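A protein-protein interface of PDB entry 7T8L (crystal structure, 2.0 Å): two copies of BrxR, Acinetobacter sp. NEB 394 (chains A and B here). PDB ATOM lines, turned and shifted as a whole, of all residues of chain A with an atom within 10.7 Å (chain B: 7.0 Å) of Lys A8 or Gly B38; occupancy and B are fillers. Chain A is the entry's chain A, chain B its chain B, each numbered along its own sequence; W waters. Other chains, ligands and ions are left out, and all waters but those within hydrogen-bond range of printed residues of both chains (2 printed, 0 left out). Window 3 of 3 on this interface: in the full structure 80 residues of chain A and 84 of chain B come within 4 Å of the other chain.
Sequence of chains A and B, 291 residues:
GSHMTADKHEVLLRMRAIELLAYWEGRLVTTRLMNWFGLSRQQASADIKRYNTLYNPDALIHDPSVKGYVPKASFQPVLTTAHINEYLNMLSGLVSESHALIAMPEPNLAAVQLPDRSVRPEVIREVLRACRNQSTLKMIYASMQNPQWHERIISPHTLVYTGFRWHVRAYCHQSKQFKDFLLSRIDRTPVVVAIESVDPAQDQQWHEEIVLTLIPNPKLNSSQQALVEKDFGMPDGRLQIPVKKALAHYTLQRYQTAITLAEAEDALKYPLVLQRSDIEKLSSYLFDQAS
The side-chain amino group of Lys A8 lies within hydrogen-bond range of the backbone carbonyl oxygen of Gly B38 (3.2 Å).
Among the printed residues, merely in contact across the chains: Lys A8 with Phe B37 (3.4 Å), His A9 with Trp B36 (3.5 Å) and His A9 with Phe B37 (3.97 Å).
Lys A8 touches two residues of chain B. Gly B38 touches one residue of chain A. No residue of chain A comes within 4 Å of Leu B39. Of the printed residues of chain A, Phe B37 touches Lys A8 and His A9. Of the printed residues of chain B, His A9 touches Trp B36 and Phe B37. Printed residues of chain A within 4 Å of Trp B36: His A9 (3.5 Å). Tyr A55 touches none of the printed residues of chain B. The nearest residue of chain B that does not touch Lys A8 is Leu B39 (5.3 Å). The nearest residue of chain A that does not touch Gly B38 is His A9 (5.5 Å).
Printed residues of chain B that touch a printed residue of chain A: Trp B36, Phe B37 and Gly B38. Printed residues of chain A that touch a printed residue of chain B: Lys A8 and His A9.
Position printed for both chains: 37. Of the 4 pairs that touch across the chains among the printed residues, none has its exchanged pair printed and touching as well.
Water W2 lies within hydrogen-bond range of O of Phe B37 (2.7 Å) and N of Glu A10 (3.0 Å). Water W1 lies within hydrogen-bond range of O of Trp B36 (2.8 Å), N of His A9 (2.9 Å) and N of Gly B38 (3.4 Å).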
ATOM      1  N   ALA A   6     -19.014 -16.915  -6.123  1.00  0.00           N
ATOM      2  CA  ALA A   6     -19.830 -17.781  -7.038  1.00  0.00           C
ATOM      3  C   ALA A   6     -19.827 -17.224  -8.471  1.00  0.00           C
ATOM      4  O   ALA A   6     -19.854 -18.058  -9.417  1.00  0.00           O
ATOM      5  CB  ALA A   6     -21.243 -17.909  -6.521  1.00  0.00           C
ATOM      6  N   ASP A   7     -19.758 -15.891  -8.627  1.00  0.00           N
ATOM      7  CA  ASP A   7     -20.176 -15.173  -9.864  1.00  0.00           C
ATOM      8  C   ASP A   7     -19.072 -15.149 -10.936  1.00  0.00           C
ATOM      9  O   ASP A   7     -17.951 -14.641 -10.713  1.00  0.00           O
ATOM     10  CB  ASP A   7     -20.712 -13.783  -9.523  1.00  0.00           C
ATOM     11  CG  ASP A   7     -22.028 -13.852  -8.767  1.00  0.00           C
ATOM     12  OD1 ASP A   7     -22.704 -14.913  -8.848  1.00  0.00           O
ATOM     13  OD2 ASP A   7     -22.377 -12.847  -8.111  1.00  0.00           O
ATOM     14  N   LYS A   8     -19.431 -15.659 -12.106  1.00  0.00           N
ATOM     15  CA  LYS A   8     -18.620 -15.622 -13.346  1.00  0.00           C
ATOM     16  C   LYS A   8     -18.698 -14.233 -14.003  1.00  0.00           C
ATOM     17  O   LYS A   8     -19.531 -13.406 -13.588  1.00  0.00           O
ATOM     18  CB  LYS A   8     -19.155 -16.686 -14.309  1.00  0.00           C
ATOM     19  CG  LYS A   8     -18.518 -18.063 -14.165  1.00  0.00           C
ATOM     20  CD  LYS A   8     -18.675 -18.722 -12.812  1.00  0.00           C
ATOM     21  CE  LYS A   8     -18.361 -20.209 -12.841  1.00  0.00           C
ATOM     22  NZ  LYS A   8     -19.465 -20.999 -13.439  1.00  0.00           N
ATOM     23  N   HIS A   9     -17.904 -14.046 -15.059  1.00  0.00           N
ATOM     24  CA  HIS A   9     -17.714 -12.772 -15.800  1.00  0.00           C
ATOM     25  C   HIS A   9     -19.061 -12.109 -16.073  1.00  0.00           C
ATOM     26  O   HIS A   9     -19.187 -10.969 -15.663  1.00  0.00           O
ATOM     27  CB  HIS A   9     -16.903 -12.966 -17.083  1.00  0.00           C
ATOM     28  CG  HIS A   9     -16.682 -11.678 -17.798  1.00  0.00           C
ATOM     29  ND1 HIS A   9     -17.501 -11.269 -18.846  1.00  0.00           N
ATOM     30  CD2 HIS A   9     -15.832 -10.662 -17.551  1.00  0.00           C
ATOM     31  CE1 HIS A   9     -17.111 -10.073 -19.249  1.00  0.00           C
ATOM     32  NE2 HIS A   9     -16.083  -9.686 -18.485  1.00  0.00           N
ATOM     33  N   GLU A  10     -20.036 -12.805 -16.669  1.00  0.00           N
ATOM     34  CA  GLU A  10     -21.249 -12.128 -17.193  1.00  0.00           C
ATOM     35  C   GLU A  10     -22.077 -11.537 -16.037  1.00  0.00           C
ATOM     36  O   GLU A  10     -22.521 -10.396 -16.169  1.00  0.00           O
ATOM     37  CB  GLU A  10     -22.087 -13.070 -18.058  1.00  0.00           C
ATOM     38  CG  GLU A  10     -23.255 -12.353 -18.719  1.00  0.00           C
ATOM     39  CD  GLU A  10     -22.923 -11.245 -19.722  1.00  0.00           C
ATOM     40  OE1 GLU A  10     -21.813 -11.272 -20.360  1.00  0.00           O
ATOM     41  OE2 GLU A  10     -23.787 -10.356 -19.881  1.00  0.00           O
ATOM     42  N   VAL A  11     -22.247 -12.272 -14.940  1.00  0.00           N
ATOM     43  CA  VAL A  11     -22.951 -11.804 -13.701  1.00  0.00           C
ATOM     44  C   VAL A  11     -22.152 -10.651 -13.062  1.00  0.00           C
ATOM     45  O   VAL A  11     -22.774  -9.614 -12.704  1.00  0.00           O
ATOM     46  CB  VAL A  11     -23.190 -12.971 -12.723  1.00  0.00           C
ATOM     47  CG1 VAL A  11     -23.777 -12.509 -11.389  1.00  0.00           C
ATOM     48  CG2 VAL A  11     -24.070 -14.035 -13.356  1.00  0.00           C
ATOM     49  N   LEU A  12     -20.834 -10.788 -12.956  1.00  0.00           N
ATOM     50  CA  LEU A  12     -19.953  -9.729 -12.396  1.00  0.00           C
ATOM     51  C   LEU A  12     -20.079  -8.450 -13.251  1.00  0.00           C
ATOM     52  O   LEU A  12     -20.087  -7.375 -12.667  1.00  0.00           O
ATOM     53  CB  LEU A  12     -18.505 -10.220 -12.335  1.00  0.00           C
ATOM     54  CG  LEU A  12     -17.683  -9.737 -11.136  1.00  0.00           C
ATOM     55  CD1 LEU A  12     -18.467  -9.847  -9.830  1.00  0.00           C
ATOM     56  CD2 LEU A  12     -16.381 -10.520 -11.027  1.00  0.00           C
ATOM     57  N   LEU A  13     -20.252  -8.572 -14.569  1.00  0.00           N
ATOM     58  CA  LEU A  13     -20.454  -7.399 -15.475  1.00  0.00           C
ATOM     59  C   LEU A  13     -21.752  -6.664 -15.108  1.00  0.00           C
ATOM     60  O   LEU A  13     -21.716  -5.429 -15.025  1.00  0.00           O
ATOM     61  CB  LEU A  13     -20.482  -7.883 -16.926  1.00  0.00           C
ATOM     62  CG  LEU A  13     -20.033  -6.872 -17.981  1.00  0.00           C
ATOM     63  CD1 LEU A  13     -18.686  -6.259 -17.620  1.00  0.00           C
ATOM     64  CD2 LEU A  13     -19.952  -7.536 -19.358  1.00  0.00           C
ATOM     65  N   ARG A  14     -22.842  -7.400 -14.873  1.00  0.00           N
ATOM     66  CA  ARG A  14     -24.153  -6.857 -14.444  1.00  0.00           C
ATOM     67  C   ARG A  14     -24.037  -6.183 -13.075  1.00  0.00           C
ATOM     68  O   ARG A  14     -24.623  -5.119 -12.860  1.00  0.00           O
ATOM     69  CB  ARG A  14     -25.230  -7.938 -14.499  1.00  0.00           C
ATOM     70  CG  ARG A  14     -25.214  -8.726 -15.799  1.00  0.00           C
ATOM     71  CD  ARG A  14     -26.553  -9.047 -16.364  1.00  0.00           C
ATOM     72  NE  ARG A  14     -27.284  -9.977 -15.511  1.00  0.00           N
ATOM     73  CZ  ARG A  14     -27.247 -11.303 -15.577  1.00  0.00           C
ATOM     74  NH1 ARG A  14     -26.453 -11.921 -16.429  1.00  0.00           N
ATOM     75  NH2 ARG A  14     -27.983 -12.014 -14.736  1.00  0.00           N
ATOM     76  N   MET A  15     -23.287  -6.785 -12.150  1.00  0.00           N
ATOM     77  CA  MET A  15     -23.101  -6.197 -10.830  1.00  0.00           C
ATOM     78  C   MET A  15     -22.327  -4.876 -10.948  1.00  0.00           C
ATOM     79  O   MET A  15     -22.678  -3.908 -10.252  1.00  0.00           O
ATOM     80  CB  MET A  15     -22.305  -7.126  -9.907  1.00  0.00           C
ATOM     81  CG  MET A  15     -22.983  -8.479  -9.547  1.00  0.00           C
ATOM     82  SD  MET A  15     -24.825  -8.376  -8.875  1.00  0.00           S
ATOM     83  CE  MET A  15     -25.951  -8.644 -10.434  1.00  0.00           C
ATOM     84  N   ARG A  16     -21.196  -4.891 -11.693  1.00  0.00           N
ATOM     85  CA  ARG A  16     -20.410  -3.679 -11.901  1.00  0.00           C
ATOM     86  C   ARG A  16     -21.302  -2.602 -12.540  1.00  0.00           C
ATOM     87  O   ARG A  16     -21.152  -1.444 -12.159  1.00  0.00           O
ATOM     88  CB  ARG A  16     -19.165  -3.892 -12.770  1.00  0.00           C
ATOM     89  CG  ARG A  16     -18.065  -4.730 -12.126  1.00  0.00           C
ATOM     90  CD  ARG A  16     -16.968  -5.118 -13.112  1.00  0.00           C
ATOM     91  NE  ARG A  16     -16.334  -3.939 -13.697  1.00  0.00           N
ATOM     92  CZ  ARG A  16     -15.270  -3.317 -13.190  1.00  0.00           C
ATOM     93  NH1 ARG A  16     -14.682  -3.782 -12.097  1.00  0.00           N
ATOM     94  NH2 ARG A  16     -14.788  -2.234 -13.779  1.00  0.00           N
ATOM     95  N   PHE A  37     -28.424  -5.667 -21.202  1.00  0.00           N
ATOM     96  CA  PHE A  37     -28.086  -7.105 -21.118  1.00  0.00           C
ATOM     97  C   PHE A  37     -29.202  -7.983 -21.701  1.00  0.00           C
ATOM     98  O   PHE A  37     -29.009  -9.206 -21.745  1.00  0.00           O
ATOM     99  CB  PHE A  37     -27.733  -7.428 -19.668  1.00  0.00           C
ATOM    100  CG  PHE A  37     -26.555  -6.646 -19.151  1.00  0.00           C
ATOM    101  CD1 PHE A  37     -25.266  -6.965 -19.548  1.00  0.00           C
ATOM    102  CD2 PHE A  37     -26.730  -5.625 -18.225  1.00  0.00           C
ATOM    103  CE1 PHE A  37     -24.176  -6.264 -19.057  1.00  0.00           C
ATOM    104  CE2 PHE A  37     -25.641  -4.917 -17.742  1.00  0.00           C
ATOM    105  CZ  PHE A  37     -24.366  -5.226 -18.171  1.00  0.00           C
ATOM    106  N   ASP A  47     -31.260  -9.096 -10.408  1.00  0.00           N
ATOM    107  CA  ASP A  47     -29.844  -8.613 -10.414  1.00  0.00           C
ATOM    108  C   ASP A  47     -29.668  -7.513  -9.361  1.00  0.00           C
ATOM    109  O   ASP A  47     -28.684  -7.554  -8.590  1.00  0.00           O
ATOM    110  CB  ASP A  47     -29.423  -8.146 -11.807  1.00  0.00           C
ATOM    111  CG  ASP A  47     -29.285  -9.268 -12.823  1.00  0.00           C
ATOM    112  OD1 ASP A  47     -29.112 -10.447 -12.413  1.00  0.00           O
ATOM    113  OD2 ASP A  47     -29.315  -8.953 -14.033  1.00  0.00           O
ATOM    114  N   ARG A  50     -29.717  -9.075  -5.926  1.00  0.00           N
ATOM    115  CA  ARG A  50     -28.390  -9.707  -5.682  1.00  0.00           C
ATOM    116  C   ARG A  50     -27.321  -8.667  -5.300  1.00  0.00           C
ATOM    117  O   ARG A  50     -26.512  -8.930  -4.374  1.00  0.00           O
ATOM    118  CB  ARG A  50     -27.995 -10.514  -6.921  1.00  0.00           C
ATOM    119  CG  ARG A  50     -26.691 -11.286  -6.786  1.00  0.00           C
ATOM    120  CD  ARG A  50     -26.376 -12.032  -8.075  1.00  0.00           C
ATOM    121  NE  ARG A  50     -25.441 -13.124  -7.862  1.00  0.00           N
ATOM    122  CZ  ARG A  50     -25.772 -14.303  -7.337  1.00  0.00           C
ATOM    123  NH1 ARG A  50     -27.010 -14.539  -6.940  1.00  0.00           N
ATOM    124  NH2 ARG A  50     -24.852 -15.233  -7.190  1.00  0.00           N
ATOM    125  N   TYR A  55     -23.531  -8.192  -2.440  1.00  0.00           N
ATOM    126  CA  TYR A  55     -22.343  -7.349  -2.751  1.00  0.00           C
ATOM    127  C   TYR A  55     -22.279  -6.101  -1.875  1.00  0.00           C
ATOM    128  O   TYR A  55     -21.196  -5.855  -1.368  1.00  0.00           O
ATOM    129  CB  TYR A  55     -22.317  -6.922  -4.220  1.00  0.00           C
ATOM    130  CG  TYR A  55     -21.916  -8.043  -5.138  1.00  0.00           C
ATOM    131  CD1 TYR A  55     -22.873  -8.904  -5.652  1.00  0.00           C
ATOM    132  CD2 TYR A  55     -20.586  -8.258  -5.465  1.00  0.00           C
ATOM    133  CE1 TYR A  55     -22.516  -9.974  -6.456  1.00  0.00           C
ATOM    134  CE2 TYR A  55     -20.215  -9.305  -6.296  1.00  0.00           C
ATOM    135  CZ  TYR A  55     -21.185 -10.166  -6.783  1.00  0.00           C
ATOM    136  OH  TYR A  55     -20.844 -11.189  -7.624  1.00  0.00           O
ATOM    137  N   LEU A  79     -16.932  -2.876  -5.944  1.00  0.00           N
ATOM    138  CA  LEU A  79     -16.392  -3.615  -7.114  1.00  0.00           C
ATOM    139  C   LEU A  79     -15.474  -2.727  -7.963  1.00  0.00           C
ATOM    140  O   LEU A  79     -14.779  -3.284  -8.811  1.00  0.00           O
ATOM    141  CB  LEU A  79     -17.580  -4.114  -7.941  1.00  0.00           C
ATOM    142  CG  LEU A  79     -18.355  -5.289  -7.348  1.00  0.00           C
ATOM    143  CD1 LEU A  79     -19.648  -5.528  -8.108  1.00  0.00           C
ATOM    144  CD2 LEU A  79     -17.504  -6.548  -7.363  1.00  0.00           C
ATOM    145  N   ARG B  32      -9.313 -21.291 -23.027  1.00  0.00           N
ATOM    146  CA  ARG B  32      -9.235 -19.811 -22.889  1.00  0.00           C
ATOM    147  C   ARG B  32     -10.635 -19.270 -22.606  1.00  0.00           C
ATOM    148  O   ARG B  32     -10.772 -18.353 -21.727  1.00  0.00           O
ATOM    149  CB  ARG B  32      -8.648 -19.172 -24.152  1.00  0.00           C
ATOM    150  CG  ARG B  32      -8.260 -17.714 -23.966  1.00  0.00           C
ATOM    151  CD  ARG B  32      -6.986 -17.552 -23.152  1.00  0.00           C
ATOM    152  NE  ARG B  32      -6.486 -16.199 -23.349  1.00  0.00           N
ATOM    153  CZ  ARG B  32      -5.867 -15.768 -24.453  1.00  0.00           C
ATOM    154  NH1 ARG B  32      -5.665 -16.579 -25.488  1.00  0.00           N
ATOM    155  NH2 ARG B  32      -5.473 -14.508 -24.530  1.00  0.00           N
ATOM    156  N   LEU B  33     -11.631 -19.767 -23.347  1.00  0.00           N
ATOM    157  CA  LEU B  33     -13.059 -19.337 -23.225  1.00  0.00           C
ATOM    158  C   LEU B  33     -13.601 -19.724 -21.852  1.00  0.00           C
ATOM    159  O   LEU B  33     -14.269 -18.927 -21.182  1.00  0.00           O
ATOM    160  CB  LEU B  33     -13.902 -19.990 -24.321  1.00  0.00           C
ATOM    161  CG  LEU B  33     -13.730 -19.410 -25.721  1.00  0.00           C
ATOM    162  CD1 LEU B  33     -14.743 -20.068 -26.670  1.00  0.00           C
ATOM    163  CD2 LEU B  33     -13.893 -17.890 -25.723  1.00  0.00           C
ATOM    164  N   MET B  34     -13.289 -20.964 -21.455  1.00  0.00           N
ATOM    165  CA  MET B  34     -13.607 -21.471 -20.126  1.00  0.00           C
ATOM    166  C   MET B  34     -13.046 -20.562 -19.039  1.00  0.00           C
ATOM    167  O   MET B  34     -13.754 -20.242 -18.105  1.00  0.00           O
ATOM    168  CB  MET B  34     -13.043 -22.888 -19.936  1.00  0.00           C
ATOM    169  CG  MET B  34     -13.764 -23.944 -20.737  1.00  0.00           C
ATOM    170  SD  MET B  34     -12.774 -25.655 -20.772  1.00  0.00           S
ATOM    171  CE  MET B  34     -13.066 -26.253 -18.909  1.00  0.00           C
ATOM    172  N   ASN B  35     -11.765 -20.205 -19.114  1.00  0.00           N
ATOM    173  CA  ASN B  35     -11.179 -19.362 -18.090  1.00  0.00           C
ATOM    174  C   ASN B  35     -11.784 -17.933 -18.134  1.00  0.00           C
ATOM    175  O   ASN B  35     -12.064 -17.369 -17.069  1.00  0.00           O
ATOM    176  CB  ASN B  35      -9.659 -19.371 -18.207  1.00  0.00           C
ATOM    177  CG  ASN B  35      -9.072 -20.747 -17.950  1.00  0.00           C
ATOM    178  OD1 ASN B  35      -9.752 -21.637 -17.444  1.00  0.00           O
ATOM    179  ND2 ASN B  35      -7.812 -20.939 -18.310  1.00  0.00           N
ATOM    180  N   TRP B  36     -11.979 -17.344 -19.313  1.00  0.00           N
ATOM    181  CA  TRP B  36     -12.585 -15.992 -19.455  1.00  0.00           C
ATOM    182  C   TRP B  36     -14.009 -15.955 -18.885  1.00  0.00           C
ATOM    183  O   TRP B  36     -14.284 -15.042 -18.088  1.00  0.00           O
ATOM    184  CB  TRP B  36     -12.543 -15.550 -20.918  1.00  0.00           C
ATOM    185  CG  TRP B  36     -11.201 -15.047 -21.361  1.00  0.00           C
ATOM    186  CD1 TRP B  36     -10.010 -15.131 -20.693  1.00  0.00           C
ATOM    187  CD2 TRP B  36     -10.908 -14.415 -22.618  1.00  0.00           C
ATOM    188  NE1 TRP B  36      -9.016 -14.539 -21.419  1.00  0.00           N
ATOM    189  CE2 TRP B  36      -9.537 -14.086 -22.603  1.00  0.00           C
ATOM    190  CE3 TRP B  36     -11.684 -14.025 -23.714  1.00  0.00           C
ATOM    191  CZ2 TRP B  36      -8.925 -13.431 -23.667  1.00  0.00           C
ATOM    192  CZ3 TRP B  36     -11.072 -13.382 -24.772  1.00  0.00           C
ATOM    193  CH2 TRP B  36      -9.716 -13.060 -24.728  1.00  0.00           C
ATOM    194  N   PHE B  37     -14.912 -16.861 -19.285  1.00  0.00           N
ATOM    195  CA  PHE B  37     -16.368 -16.764 -19.009  1.00  0.00           C
ATOM    196  C   PHE B  37     -16.849 -17.749 -17.922  1.00  0.00           C
ATOM    197  O   PHE B  37     -18.004 -17.619 -17.542  1.00  0.00           O
ATOM    198  CB  PHE B  37     -17.156 -16.937 -20.306  1.00  0.00           C
ATOM    199  CG  PHE B  37     -16.838 -15.872 -21.318  1.00  0.00           C
ATOM    200  CD1 PHE B  37     -17.269 -14.562 -21.121  1.00  0.00           C
ATOM    201  CD2 PHE B  37     -16.051 -16.157 -22.428  1.00  0.00           C
ATOM    202  CE1 PHE B  37     -16.938 -13.569 -22.034  1.00  0.00           C
ATOM    203  CE2 PHE B  37     -15.707 -15.156 -23.322  1.00  0.00           C
ATOM    204  CZ  PHE B  37     -16.163 -13.869 -23.130  1.00  0.00           C
ATOM    205  N   GLY B  38     -16.009 -18.662 -17.425  1.00  0.00           N
ATOM    206  CA  GLY B  38     -16.394 -19.753 -16.495  1.00  0.00           C
ATOM    207  C   GLY B  38     -17.421 -20.709 -17.093  1.00  0.00           C
ATOM    208  O   GLY B  38     -18.318 -21.122 -16.383  1.00  0.00           O
ATOM    209  N   LEU B  39     -17.287 -21.044 -18.374  1.00  0.00           N
ATOM    210  CA  LEU B  39     -18.142 -22.011 -19.094  1.00  0.00           C
ATOM    211  C   LEU B  39     -17.604 -23.408 -18.823  1.00  0.00           C
ATOM    212  O   LEU B  39     -16.410 -23.546 -18.578  1.00  0.00           O
ATOM    213  CB  LEU B  39     -18.076 -21.764 -20.606  1.00  0.00           C
ATOM    214  CG  LEU B  39     -18.336 -20.336 -21.076  1.00  0.00           C
ATOM    215  CD1 LEU B  39     -18.148 -20.235 -22.585  1.00  0.00           C
ATOM    216  CD2 LEU B  39     -19.724 -19.894 -20.649  1.00  0.00           C
ATOM    217  N   SER B  40     -18.445 -24.413 -18.994  1.00  0.00           N
ATOM    218  CA  SER B  40     -18.002 -25.819 -19.161  1.00  0.00           C
ATOM    219  C   SER B  40     -17.284 -25.958 -20.511  1.00  0.00           C
ATOM    220  O   SER B  40     -17.525 -25.121 -21.430  1.00  0.00           O
ATOM    221  CB  SER B  40     -19.181 -26.733 -19.061  1.00  0.00           C
ATOM    222  OG  SER B  40     -20.116 -26.433 -20.088  1.00  0.00           O
HETATM  223  O   HOH W   1     -15.662 -15.775 -15.704  1.00  0.00           O
HETATM  224  O   HOH W   2     -19.751 -15.569 -17.837  1.00  0.00           O
